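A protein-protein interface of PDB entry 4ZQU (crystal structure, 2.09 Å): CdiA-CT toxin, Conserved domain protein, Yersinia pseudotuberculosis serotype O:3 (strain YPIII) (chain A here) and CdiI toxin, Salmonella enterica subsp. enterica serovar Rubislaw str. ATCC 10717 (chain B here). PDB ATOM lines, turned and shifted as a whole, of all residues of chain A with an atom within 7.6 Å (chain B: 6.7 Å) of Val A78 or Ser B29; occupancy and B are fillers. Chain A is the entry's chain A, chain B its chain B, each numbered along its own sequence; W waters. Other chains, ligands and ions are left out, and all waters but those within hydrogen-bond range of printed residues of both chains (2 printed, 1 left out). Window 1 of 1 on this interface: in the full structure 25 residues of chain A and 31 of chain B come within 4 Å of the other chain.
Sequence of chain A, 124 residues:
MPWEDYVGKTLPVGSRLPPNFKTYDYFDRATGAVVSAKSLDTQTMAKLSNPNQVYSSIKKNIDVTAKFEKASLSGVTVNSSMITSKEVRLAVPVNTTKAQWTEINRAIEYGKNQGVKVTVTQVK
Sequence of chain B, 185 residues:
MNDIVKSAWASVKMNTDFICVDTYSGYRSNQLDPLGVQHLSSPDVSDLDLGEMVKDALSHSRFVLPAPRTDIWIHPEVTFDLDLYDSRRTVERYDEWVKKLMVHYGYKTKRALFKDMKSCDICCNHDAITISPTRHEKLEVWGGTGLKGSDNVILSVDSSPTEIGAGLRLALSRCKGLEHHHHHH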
ATOM      1  N   GLY A  14      13.420 -16.517   1.335  1.00  0.00           N
ATOM      2  CA  GLY A  14      14.801 -16.529   0.888  1.00  0.00           C
ATOM      3  C   GLY A  14      15.194 -15.271   0.139  1.00  0.00           C
ATOM      4  O   GLY A  14      16.309 -15.170  -0.370  1.00  0.00           O
ATOM      5  N   LEU A  17      18.150 -10.176   1.736  1.00  0.00           N
ATOM      6  CA  LEU A  17      19.595 -10.067   1.628  1.00  0.00           C
ATOM      7  C   LEU A  17      20.202  -9.756   2.989  1.00  0.00           C
ATOM      8  O   LEU A  17      19.537  -9.165   3.842  1.00  0.00           O
ATOM      9  CB  LEU A  17      19.967  -8.983   0.618  1.00  0.00           C
ATOM     10  CG  LEU A  17      19.624  -9.289  -0.839  1.00  0.00           C
ATOM     11  CD1 LEU A  17      19.693  -8.023  -1.664  1.00  0.00           C
ATOM     12  CD2 LEU A  17      20.572 -10.338  -1.385  1.00  0.00           C
ATOM     13  N   PRO A  18      21.466 -10.158   3.202  1.00  0.00           N
ATOM     14  CA  PRO A  18      22.150  -9.842   4.460  1.00  0.00           C
ATOM     15  C   PRO A  18      22.249  -8.334   4.658  1.00  0.00           C
ATOM     16  O   PRO A  18      22.322  -7.602   3.670  1.00  0.00           O
ATOM     17  CB  PRO A  18      23.534 -10.476   4.280  1.00  0.00           C
ATOM     18  CG  PRO A  18      23.712 -10.590   2.801  1.00  0.00           C
ATOM     19  CD  PRO A  18      22.345 -10.886   2.270  1.00  0.00           C
ATOM     20  N   PHE A  21      23.315  -4.552   2.453  1.00  0.00           N
ATOM     21  CA  PHE A  21      23.722  -4.962   1.114  1.00  0.00           C
ATOM     22  C   PHE A  21      23.492  -3.812   0.141  1.00  0.00           C
ATOM     23  O   PHE A  21      22.556  -3.847  -0.665  1.00  0.00           O
ATOM     24  CB  PHE A  21      22.956  -6.201   0.654  1.00  0.00           C
ATOM     25  CG  PHE A  21      23.662  -6.980  -0.418  1.00  0.00           C
ATOM     26  CD1 PHE A  21      24.381  -8.118  -0.096  1.00  0.00           C
ATOM     27  CD2 PHE A  21      23.619  -6.570  -1.743  1.00  0.00           C
ATOM     28  CE1 PHE A  21      25.037  -8.839  -1.072  1.00  0.00           C
ATOM     29  CE2 PHE A  21      24.275  -7.289  -2.727  1.00  0.00           C
ATOM     30  CZ  PHE A  21      24.985  -8.425  -2.390  1.00  0.00           C
ATOM     31  N   TYR A  24      19.937  -2.560  -1.531  1.00  0.00           N
ATOM     32  CA  TYR A  24      19.005  -3.661  -1.755  1.00  0.00           C
ATOM     33  C   TYR A  24      18.768  -4.471  -0.486  1.00  0.00           C
ATOM     34  O   TYR A  24      19.711  -4.962   0.136  1.00  0.00           O
ATOM     35  CB  TYR A  24      19.515  -4.577  -2.869  1.00  0.00           C
ATOM     36  CG  TYR A  24      19.663  -3.893  -4.210  1.00  0.00           C
ATOM     37  CD1 TYR A  24      18.860  -2.812  -4.553  1.00  0.00           C
ATOM     38  CD2 TYR A  24      20.613  -4.322  -5.126  1.00  0.00           C
ATOM     39  CE1 TYR A  24      18.995  -2.180  -5.775  1.00  0.00           C
ATOM     40  CE2 TYR A  24      20.755  -3.696  -6.352  1.00  0.00           C
ATOM     41  CZ  TYR A  24      19.944  -2.625  -6.670  1.00  0.00           C
ATOM     42  OH  TYR A  24      20.080  -1.998  -7.889  1.00  0.00           O
ATOM     43  N   PHE A  27      15.810  -9.653  -2.593  1.00  0.00           N
ATOM     44  CA  PHE A  27      16.125 -10.095  -3.939  1.00  0.00           C
ATOM     45  C   PHE A  27      15.335 -11.351  -4.264  1.00  0.00           C
ATOM     46  O   PHE A  27      15.533 -12.389  -3.635  1.00  0.00           O
ATOM     47  CB  PHE A  27      17.626 -10.355  -4.082  1.00  0.00           C
ATOM     48  CG  PHE A  27      18.060 -10.678  -5.486  1.00  0.00           C
ATOM     49  CD1 PHE A  27      17.533  -9.993  -6.563  1.00  0.00           C
ATOM     50  CD2 PHE A  27      18.997 -11.666  -5.727  1.00  0.00           C
ATOM     51  CE1 PHE A  27      17.933 -10.284  -7.856  1.00  0.00           C
ATOM     52  CE2 PHE A  27      19.397 -11.963  -7.018  1.00  0.00           C
ATOM     53  CZ  PHE A  27      18.865 -11.270  -8.080  1.00  0.00           C
ATOM     54  N   ASP A  28      14.425 -11.255  -5.229  1.00  0.00           N
ATOM     55  CA  ASP A  28      13.704 -12.433  -5.696  1.00  0.00           C
ATOM     56  C   ASP A  28      14.697 -13.337  -6.412  1.00  0.00           C
ATOM     57  O   ASP A  28      15.120 -13.047  -7.528  1.00  0.00           O
ATOM     58  CB  ASP A  28      12.543 -12.042  -6.615  1.00  0.00           C
ATOM     59  CG  ASP A  28      11.604 -13.203  -6.906  1.00  0.00           C
ATOM     60  OD1 ASP A  28      12.090 -14.330  -7.141  1.00  0.00           O
ATOM     61  OD2 ASP A  28      10.375 -12.987  -6.906  1.00  0.00           O
ATOM     62  N   ARG A  29      15.067 -14.434  -5.762  1.00  0.00           N
ATOM     63  CA  ARG A  29      16.153 -15.280  -6.241  1.00  0.00           C
ATOM     64  C   ARG A  29      15.820 -15.981  -7.551  1.00  0.00           C
ATOM     65  O   ARG A  29      16.708 -16.522  -8.208  1.00  0.00           O
ATOM     66  CB  ARG A  29      16.522 -16.319  -5.182  1.00  0.00           C
ATOM     67  CG  ARG A  29      16.733 -15.741  -3.796  1.00  0.00           C
ATOM     68  CD  ARG A  29      17.773 -14.630  -3.784  1.00  0.00           C
ATOM     69  NE  ARG A  29      17.899 -14.058  -2.448  1.00  0.00           N
ATOM     70  CZ  ARG A  29      19.009 -14.089  -1.720  1.00  0.00           C
ATOM     71  NH1 ARG A  29      20.108 -14.646  -2.203  1.00  0.00           N
ATOM     72  NH2 ARG A  29      19.023 -13.551  -0.509  1.00  0.00           N
ATOM     73  N   ALA A  30      14.547 -15.968  -7.932  1.00  0.00           N
ATOM     74  CA  ALA A  30      14.123 -16.630  -9.160  1.00  0.00           C
ATOM     75  C   ALA A  30      13.860 -15.648 -10.305  1.00  0.00           C
ATOM     76  O   ALA A  30      14.278 -15.890 -11.438  1.00  0.00           O
ATOM     77  CB  ALA A  30      12.889 -17.470  -8.897  1.00  0.00           C
ATOM     78  N   GLY A  32      14.526 -12.110 -10.238  1.00  0.00           N
ATOM     79  CA  GLY A  32      15.552 -11.090 -10.360  1.00  0.00           C
ATOM     80  C   GLY A  32      15.081  -9.701  -9.981  1.00  0.00           C
ATOM     81  O   GLY A  32      15.787  -8.716 -10.190  1.00  0.00           O
ATOM     82  N   VAL A  34      14.630  -6.782  -7.611  1.00  0.00           N
ATOM     83  CA  VAL A  34      15.225  -6.292  -6.371  1.00  0.00           C
ATOM     84  C   VAL A  34      14.314  -5.270  -5.702  1.00  0.00           C
ATOM     85  O   VAL A  34      13.620  -4.504  -6.371  1.00  0.00           O
ATOM     86  CB  VAL A  34      16.618  -5.658  -6.591  1.00  0.00           C
ATOM     87  CG1 VAL A  34      17.574  -6.668  -7.178  1.00  0.00           C
ATOM     88  CG2 VAL A  34      16.527  -4.437  -7.481  1.00  0.00           C
ATOM     89  N   PHE A  68      23.575   0.710  -9.675  1.00  0.00           N
ATOM     90  CA  PHE A  68      24.134  -0.521  -9.135  1.00  0.00           C
ATOM     91  C   PHE A  68      24.703  -1.408 -10.239  1.00  0.00           C
ATOM     92  O   PHE A  68      23.998  -1.772 -11.183  1.00  0.00           O
ATOM     93  CB  PHE A  68      23.070  -1.282  -8.345  1.00  0.00           C
ATOM     94  CG  PHE A  68      23.549  -2.588  -7.784  1.00  0.00           C
ATOM     95  CD1 PHE A  68      24.106  -2.647  -6.521  1.00  0.00           C
ATOM     96  CD2 PHE A  68      23.437  -3.759  -8.518  1.00  0.00           C
ATOM     97  CE1 PHE A  68      24.543  -3.843  -6.002  1.00  0.00           C
ATOM     98  CE2 PHE A  68      23.876  -4.958  -8.004  1.00  0.00           C
ATOM     99  CZ  PHE A  68      24.430  -5.000  -6.743  1.00  0.00           C
ATOM    100  N   GLU A  69      25.979  -1.757 -10.111  1.00  0.00           N
ATOM    101  CA  GLU A  69      26.629  -2.660 -11.054  1.00  0.00           C
ATOM    102  C   GLU A  69      26.855  -4.033 -10.429  1.00  0.00           C
ATOM    103  O   GLU A  69      26.484  -5.059 -11.003  1.00  0.00           O
ATOM    104  CB  GLU A  69      27.963  -2.078 -11.528  1.00  0.00           C
ATOM    105  CG  GLU A  69      28.789  -3.041 -12.376  1.00  0.00           C
ATOM    106  CD  GLU A  69      30.126  -2.458 -12.788  1.00  0.00           C
ATOM    107  OE1 GLU A  69      30.383  -1.280 -12.462  1.00  0.00           O
ATOM    108  OE2 GLU A  69      30.920  -3.175 -13.435  1.00  0.00           O
ATOM    109  N   LYS A  70      27.464  -4.043  -9.249  1.00  0.00           N
ATOM    110  CA  LYS A  70      27.803  -5.285  -8.570  1.00  0.00           C
ATOM    111  C   LYS A  70      28.128  -5.031  -7.102  1.00  0.00           C
ATOM    112  O   LYS A  70      28.746  -4.022  -6.763  1.00  0.00           O
ATOM    113  CB  LYS A  70      28.986  -5.966  -9.270  1.00  0.00           C
ATOM    114  CG  LYS A  70      29.438  -7.266  -8.627  1.00  0.00           C
ATOM    115  CD  LYS A  70      30.320  -8.079  -9.565  1.00  0.00           C
ATOM    116  CE  LYS A  70      31.620  -7.363  -9.889  1.00  0.00           C
ATOM    117  NZ  LYS A  70      32.546  -8.230 -10.672  1.00  0.00           N
ATOM    118  N   ALA A  71      27.687  -5.938  -6.235  1.00  0.00           N
ATOM    119  CA  ALA A  71      28.038  -5.892  -4.819  1.00  0.00           C
ATOM    120  C   ALA A  71      28.310  -7.297  -4.301  1.00  0.00           C
ATOM    121  O   ALA A  71      27.538  -8.220  -4.554  1.00  0.00           O
ATOM    122  CB  ALA A  71      26.935  -5.232  -4.006  1.00  0.00           C
ATOM    123  N   SER A  72      29.415  -7.452  -3.582  1.00  0.00           N
ATOM    124  CA  SER A  72      29.793  -8.737  -3.009  1.00  0.00           C
ATOM    125  C   SER A  72      30.221  -8.549  -1.561  1.00  0.00           C
ATOM    126  O   SER A  72      31.257  -7.941  -1.284  1.00  0.00           O
ATOM    127  CB  SER A  72      30.917  -9.387  -3.821  1.00  0.00           C
ATOM    128  OG  SER A  72      31.194 -10.702  -3.362  1.00  0.00           O
ATOM    129  N   LEU A  73      29.416  -9.069  -0.642  1.00  0.00           N
ATOM    130  CA  LEU A  73      29.652  -8.867   0.781  1.00  0.00           C
ATOM    131  C   LEU A  73      28.907  -9.910   1.608  1.00  0.00           C
ATOM    132  O   LEU A  73      27.880 -10.429   1.176  1.00  0.00           O
ATOM    133  CB  LEU A  73      29.228  -7.454   1.190  1.00  0.00           C
ATOM    134  CG  LEU A  73      27.766  -7.074   0.935  1.00  0.00           C
ATOM    135  CD1 LEU A  73      26.991  -6.996   2.244  1.00  0.00           C
ATOM    136  CD2 LEU A  73      27.661  -5.765   0.162  1.00  0.00           C
ATOM    137  N   VAL A  76      27.973 -13.132  -0.110  1.00  0.00           N
ATOM    138  CA  VAL A  76      26.942 -13.116  -1.148  1.00  0.00           C
ATOM    139  C   VAL A  76      27.319 -12.191  -2.305  1.00  0.00           C
ATOM    140  O   VAL A  76      27.807 -11.081  -2.089  1.00  0.00           O
ATOM    141  CB  VAL A  76      25.576 -12.672  -0.579  1.00  0.00           C
ATOM    142  CG1 VAL A  76      24.495 -12.709  -1.660  1.00  0.00           C
ATOM    143  CG2 VAL A  76      25.182 -13.545   0.600  1.00  0.00           C
ATOM    144  N   THR A  77      27.083 -12.651  -3.533  1.00  0.00           N
ATOM    145  CA  THR A  77      27.408 -11.873  -4.726  1.00  0.00           C
ATOM    146  C   THR A  77      26.172 -11.587  -5.581  1.00  0.00           C
ATOM    147  O   THR A  77      25.421 -12.498  -5.931  1.00  0.00           O
ATOM    148  CB  THR A  77      28.463 -12.594  -5.597  1.00  0.00           C
ATOM    149  OG1 THR A  77      29.673 -12.767  -4.847  1.00  0.00           O
ATOM    150  CG2 THR A  77      28.760 -11.789  -6.857  1.00  0.00           C
ATOM    151  N   VAL A  78      25.964 -10.312  -5.900  1.00  0.00           N
ATOM    152  CA  VAL A  78      24.878  -9.885  -6.780  1.00  0.00           C
ATOM    153  C   VAL A  78      25.392  -8.844  -7.771  1.00  0.00           C
ATOM    154  O   VAL A  78      26.101  -7.920  -7.384  1.00  0.00           O
ATOM    155  CB  VAL A  78      23.689  -9.282  -5.989  1.00  0.00           C
ATOM    156  CG1 VAL A  78      22.563  -8.880  -6.936  1.00  0.00           C
ATOM    157  CG2 VAL A  78      23.176 -10.257  -4.937  1.00  0.00           C
ATOM    158  N   ASN A  79      25.054  -8.996  -9.049  1.00  0.00           N
ATOM    159  CA  ASN A  79      25.356  -7.950 -10.020  1.00  0.00           C
ATOM    160  C   ASN A  79      24.134  -7.589 -10.859  1.00  0.00           C
ATOM    161  O   ASN A  79      23.107  -8.264 -10.797  1.00  0.00           O
ATOM    162  CB  ASN A  79      26.538  -8.347 -10.919  1.00  0.00           C
ATOM    163  CG  ASN A  79      26.292  -9.623 -11.709  1.00  0.00           C
ATOM    164  OD1 ASN A  79      25.160  -9.961 -12.047  1.00  0.00           O
ATOM    165  ND2 ASN A  79      27.368 -10.336 -12.014  1.00  0.00           N
ATOM    166  N   SER A  80      24.261  -6.525 -11.644  1.00  0.00           N
ATOM    167  CA  SER A  80      23.127  -5.951 -12.358  1.00  0.00           C
ATOM    168  C   SER A  80      22.572  -6.864 -13.448  1.00  0.00           C
ATOM    169  O   SER A  80      21.425  -6.710 -13.866  1.00  0.00           O
ATOM    170  CB  SER A  80      23.525  -4.607 -12.967  1.00  0.00           C
ATOM    171  OG  SER A  80      24.675  -4.748 -13.783  1.00  0.00           O
ATOM    172  N   SER A  81      23.384  -7.811 -13.908  1.00  0.00           N
ATOM    173  CA  SER A  81      22.958  -8.754 -14.936  1.00  0.00           C
ATOM    174  C   SER A  81      21.877  -9.692 -14.405  1.00  0.00           C
ATOM    175  O   SER A  81      21.090 -10.247 -15.173  1.00  0.00           O
ATOM    176  CB  SER A  81      24.149  -9.564 -15.449  1.00  0.00           C
ATOM    177  OG  SER A  81      24.692 -10.376 -14.423  1.00  0.00           O
ATOM    178  N   MET A  82      21.849  -9.858 -13.086  1.00  0.00           N
ATOM    179  CA  MET A  82      20.870 -10.711 -12.419  1.00  0.00           C
ATOM    180  C   MET A  82      19.545  -9.988 -12.219  1.00  0.00           C
ATOM    181  O   MET A  82      18.490 -10.611 -12.132  1.00  0.00           O
ATOM    182  CB  MET A  82      21.403 -11.175 -11.063  1.00  0.00           C
ATOM    183  CG  MET A  82      22.796 -11.773 -11.095  1.00  0.00           C
ATOM    184  SD  MET A  82      23.524 -11.872  -9.446  1.00  0.00           S
ATOM    185  CE  MET A  82      25.131 -12.570  -9.806  1.00  0.00           C
ATOM    186  N   ILE A  83      19.616  -8.664 -12.144  1.00  0.00           N
ATOM    187  CA  ILE A  83      18.468  -7.839 -11.795  1.00  0.00           C
ATOM    188  C   ILE A  83      17.563  -7.562 -12.994  1.00  0.00           C
ATOM    189  O   ILE A  83      18.017  -7.039 -14.015  1.00  0.00           O
ATOM    190  CB  ILE A  83      18.935  -6.507 -11.188  1.00  0.00           C
ATOM    191  CG1 ILE A  83      19.894  -6.771 -10.024  1.00  0.00           C
ATOM    192  CG2 ILE A  83      17.745  -5.670 -10.750  1.00  0.00           C
ATOM    193  CD1 ILE A  83      20.541  -5.524  -9.465  1.00  0.00           C
ATOM    194  N   TRP B   9      29.243 -21.682  -9.602  1.00  0.00           N
ATOM    195  CA  TRP B   9      29.950 -20.499  -9.133  1.00  0.00           C
ATOM    196  C   TRP B   9      31.084 -20.821  -8.169  1.00  0.00           C
ATOM    197  O   TRP B   9      31.195 -21.930  -7.648  1.00  0.00           O
ATOM    198  CB  TRP B   9      28.978 -19.531  -8.455  1.00  0.00           C
ATOM    199  CG  TRP B   9      27.841 -19.092  -9.322  1.00  0.00           C
ATOM    200  CD1 TRP B   9      27.806 -17.995 -10.129  1.00  0.00           C
ATOM    201  CD2 TRP B   9      26.568 -19.732  -9.457  1.00  0.00           C
ATOM    202  NE1 TRP B   9      26.590 -17.913 -10.763  1.00  0.00           N
ATOM    203  CE2 TRP B   9      25.813 -18.968 -10.369  1.00  0.00           C
ATOM    204  CE3 TRP B   9      25.995 -20.877  -8.900  1.00  0.00           C
ATOM    205  CZ2 TRP B   9      24.515 -19.313 -10.735  1.00  0.00           C
ATOM    206  CZ3 TRP B   9      24.707 -21.219  -9.265  1.00  0.00           C
ATOM    207  CH2 TRP B   9      23.980 -20.439 -10.174  1.00  0.00           C
ATOM    208  N   SER B  25      27.059 -21.036  -4.535  1.00  0.00           N
ATOM    209  CA  SER B  25      25.914 -21.710  -5.123  1.00  0.00           C
ATOM    210  C   SER B  25      24.731 -20.768  -5.228  1.00  0.00           C
ATOM    211  O   SER B  25      24.632 -19.800  -4.479  1.00  0.00           O
ATOM    212  CB  SER B  25      25.533 -22.939  -4.298  1.00  0.00           C
ATOM    213  OG  SER B  25      26.592 -23.877  -4.263  1.00  0.00           O
ATOM    214  N   GLY B  26      23.833 -21.049  -6.163  1.00  0.00           N
ATOM    215  CA  GLY B  26      22.634 -20.250  -6.295  1.00  0.00           C
ATOM    216  C   GLY B  26      21.867 -20.466  -7.579  1.00  0.00           C
ATOM    217  O   GLY B  26      21.752 -21.583  -8.080  1.00  0.00           O
ATOM    218  N   TYR B  27      21.344 -19.370  -8.112  1.00  0.00           N
ATOM    219  CA  TYR B  27      20.443 -19.396  -9.250  1.00  0.00           C
ATOM    220  C   TYR B  27      20.676 -18.134 -10.056  1.00  0.00           C
ATOM    221  O   TYR B  27      21.215 -18.171 -11.160  1.00  0.00           O
ATOM    222  CB  TYR B  27      18.998 -19.483  -8.770  1.00  0.00           C
ATOM    223  CG  TYR B  27      17.967 -19.732  -9.845  1.00  0.00           C
ATOM    224  CD1 TYR B  27      17.725 -21.013 -10.317  1.00  0.00           C
ATOM    225  CD2 TYR B  27      17.212 -18.689 -10.366  1.00  0.00           C
ATOM    226  CE1 TYR B  27      16.770 -21.248 -11.286  1.00  0.00           C
ATOM    227  CE2 TYR B  27      16.256 -18.913 -11.339  1.00  0.00           C
ATOM    228  CZ  TYR B  27      16.038 -20.194 -11.795  1.00  0.00           C
ATOM    229  OH  TYR B  27      15.088 -20.424 -12.764  1.00  0.00           O
ATOM    230  N   ARG B  28      20.264 -17.009  -9.485  1.00  0.00           N
ATOM    231  CA  ARG B  28      20.639 -15.705 -10.008  1.00  0.00           C
ATOM    232  C   ARG B  28      21.797 -15.176  -9.171  1.00  0.00           C
ATOM    233  O   ARG B  28      22.924 -15.063  -9.656  1.00  0.00           O
ATOM    234  CB  ARG B  28      19.450 -14.744  -9.997  1.00  0.00           C
ATOM    235  CG  ARG B  28      18.406 -15.078 -11.051  1.00  0.00           C
ATOM    236  CD  ARG B  28      17.351 -13.995 -11.174  1.00  0.00           C
ATOM    237  NE  ARG B  28      16.484 -14.206 -12.334  1.00  0.00           N
ATOM    238  CZ  ARG B  28      16.644 -13.609 -13.512  1.00  0.00           C
ATOM    239  NH1 ARG B  28      17.637 -12.751 -13.700  1.00  0.00           N
ATOM    240  NH2 ARG B  28      15.803 -13.867 -14.506  1.00  0.00           N
ATOM    241  N   SER B  29      21.520 -14.870  -7.908  1.00  0.00           N
ATOM    242  CA  SER B  29      22.584 -14.571  -6.959  1.00  0.00           C
ATOM    243  C   SER B  29      23.340 -15.853  -6.630  1.00  0.00           C
ATOM    244  O   SER B  29      22.804 -16.952  -6.770  1.00  0.00           O
ATOM    245  CB  SER B  29      22.020 -13.944  -5.681  1.00  0.00           C
ATOM    246  OG  SER B  29      21.184 -14.857  -4.989  1.00  0.00           O
ATOM    247  N   ASN B  30      24.589 -15.712  -6.205  1.00  0.00           N
ATOM    248  CA  ASN B  30      25.367 -16.856  -5.749  1.00  0.00           C
ATOM    249  C   ASN B  30      26.107 -16.509  -4.466  1.00  0.00           C
ATOM    250  O   ASN B  30      26.576 -15.385  -4.295  1.00  0.00           O
ATOM    251  CB  ASN B  30      26.343 -17.315  -6.833  1.00  0.00           C
ATOM    252  CG  ASN B  30      27.304 -16.223  -7.255  1.00  0.00           C
ATOM    253  OD1 ASN B  30      28.437 -16.158  -6.780  1.00  0.00           O
ATOM    254  ND2 ASN B  30      26.854 -15.354  -8.153  1.00  0.00           N
ATOM    255  N   GLN B  31      26.203 -17.470  -3.556  1.00  0.00           N
ATOM    256  CA  GLN B  31      26.752 -17.187  -2.239  1.00  0.00           C
ATOM    257  C   GLN B  31      27.503 -18.369  -1.639  1.00  0.00           C
ATOM    258  O   GLN B  31      27.344 -19.508  -2.080  1.00  0.00           O
ATOM    259  CB  GLN B  31      25.634 -16.761  -1.293  1.00  0.00           C
ATOM    260  CG  GLN B  31      24.562 -17.814  -1.087  1.00  0.00           C
ATOM    261  CD  GLN B  31      23.384 -17.281  -0.304  1.00  0.00           C
ATOM    262  OE1 GLN B  31      23.361 -17.343   0.924  1.00  0.00           O
ATOM    263  NE2 GLN B  31      22.398 -16.743  -1.014  1.00  0.00           N
ATOM    264  N   VAL B  64      20.438 -23.884  -7.244  1.00  0.00           N
ATOM    265  CA  VAL B  64      19.473 -24.032  -6.163  1.00  0.00           C
ATOM    266  C   VAL B  64      18.686 -22.747  -5.875  1.00  0.00           C
ATOM    267  O   VAL B  64      19.206 -21.641  -6.015  1.00  0.00           O
ATOM    268  CB  VAL B  64      20.207 -24.519  -4.879  1.00  0.00           C
ATOM    269  CG1 VAL B  64      21.413 -23.637  -4.584  1.00  0.00           C
ATOM    270  CG2 VAL B  64      19.272 -24.603  -3.677  1.00  0.00           C
ATOM    271  N   TYR B  85      19.845 -19.913   1.814  1.00  0.00           N
ATOM    272  CA  TYR B  85      19.386 -18.558   1.535  1.00  0.00           C
ATOM    273  C   TYR B  85      18.968 -17.773   2.780  1.00  0.00           C
ATOM    274  O   TYR B  85      18.792 -16.554   2.709  1.00  0.00           O
ATOM    275  CB  TYR B  85      18.221 -18.604   0.546  1.00  0.00           C
ATOM    276  CG  TYR B  85      18.645 -18.837  -0.887  1.00  0.00           C
ATOM    277  CD1 TYR B  85      18.682 -20.117  -1.427  1.00  0.00           C
ATOM    278  CD2 TYR B  85      19.007 -17.772  -1.702  1.00  0.00           C
ATOM    279  CE1 TYR B  85      19.069 -20.329  -2.740  1.00  0.00           C
ATOM    280  CE2 TYR B  85      19.396 -17.974  -3.012  1.00  0.00           C
ATOM    281  CZ  TYR B  85      19.423 -19.254  -3.527  1.00  0.00           C
ATOM    282  OH  TYR B  85      19.808 -19.452  -4.833  1.00  0.00           O
HETATM  283  O   HOH W   1      16.658 -14.770   2.957  1.00  0.00           O
HETATM  284  O   HOH W   2      12.861 -18.630 -12.947  1.00  0.00           O
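Of the 25 printed residues of chain A, 9 touch a printed residue of chain B. Printed residues of chain A that touch a printed residue of chain B: Gly A14, Phe A27, Arg A29, Ala A30, Gly A32, Val A76, Thr A77, Val A78 and Met A82. Hydrophobic or aromatic side chains of chain A that line the printed part of chain B: Phe A27, Val A76, Val A78 and Met A82. Printed residues of chain B that touch a printed residue of chain A: Tyr B27, Arg B28, Ser B29, Asn B30, Gln B31 and Tyr B85. Among the printed residues, 18 pairs touch across the chains.
Among the printed residues, merely in contact across the chains: Arg A29 with Tyr B27 (3.1 Å), Arg A29 with Tyr B85 (3.4 Å), Gly A32 with Arg B28 (3.5 Å), Phe A27 with Ser B29 (3.5 Å), Arg A29 with Arg B28 (3.6 Å), Ala A30 with Tyr B27 (3.6 Å), Thr A77 with Ser B29 (3.7 Å), Met A82 with Asn B30 (3.7 Å), Val A76 with Gln B31 (3.8 Å), Met A82 with Ser B29 (3.8 Å), Val A76 with Asn B30 (3.8 Å), Val A78 with Ser B29 (3.9 Å) and Gly A14 with Tyr B85 (3.98 Å).
The backbone carbonyl oxygen (O) of Phe A27 sits at hydrogen-bond distance from the guanidinium group (NE) of Arg A29 (3.1 Å). O of Val B64 lies within hydrogen-bond range of OH of Tyr B85. OG of Ser A72 lies within hydrogen-bond range of OG1 of Thr A77 (3.0 Å). The backbone carbonyl oxygen (O) of Gln B31 is in hydrogen-bond range of the backbone NH (N) of Ser B25, 2.9 Å away. O of Val A78 lies within hydrogen-bond range of N of Ala A71, 2.8 Å away. N of Asn A79 is in hydrogen-bond range of SD of Met A82, at 3.3 Å.
The guanidinium group (NH1) of Arg A29 sits close to the side-chain amide nitrogen (NE2) of Gln B31 (3.3 Å). The backbone carbonyl oxygen (O) of Met A82 sits at hydrogen-bond distance from the guanidinium group (NH1) of Arg B28 (2.8 Å). O of Ala A30 sits at hydrogen-bond distance from NE of Arg B28 (2.9 Å). The guanidinium group (NH1) of Arg A29 sits at hydrogen-bond distance from the side-chain hydroxyl (OG) of Ser B29 (3.0 Å). The backbone carbonyl oxygen (O) of Asn B30 lies within hydrogen-bond range of the backbone NH (N) of Thr A77 (2.9 Å).
Printed residues of chain B within 4 Å of Arg A29: Tyr B27 (3.1 Å), Arg B28 (3.6 Å), Ser B29 (3.0 Å), Gln B31 (3.3 Å) and Tyr B85 (3.4 Å). Of the printed residues of chain B, Ala A30 touches Tyr B27 (3.6 Å) and Arg B28 (2.9 Å). Val A78 touches one residue of chain B. Of chain A, only Phe A27 (3.5 Å), Arg A29 (3.0 Å), Thr A77 (3.7 Å), Val A78 (3.9 Å) and Met A82 (3.8 Å) come within 4 Å of Ser B29. Printed residues of chain A within 4 Å of Gln B31: Arg A29 (3.3 Å) and Val A76 (3.8 Å). Of the printed residues of chain A, Tyr B85 touches Gly A14 (3.98 Å) and Arg A29 (3.4 Å). The nearest residue of chain A that does not touch Ser B29 is Val A76 (4.9 Å).
Water W1 lies within hydrogen-bond range of the backbone carbonyl oxygen (O) of Tyr B85 (2.8 Å) and the backbone carbonyl oxygen (O) of Gly A14 (3.4 Å). Water W2 bridges OH of Tyr B27 (2.9 Å) and O of Ala A30 (3.4 Å).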
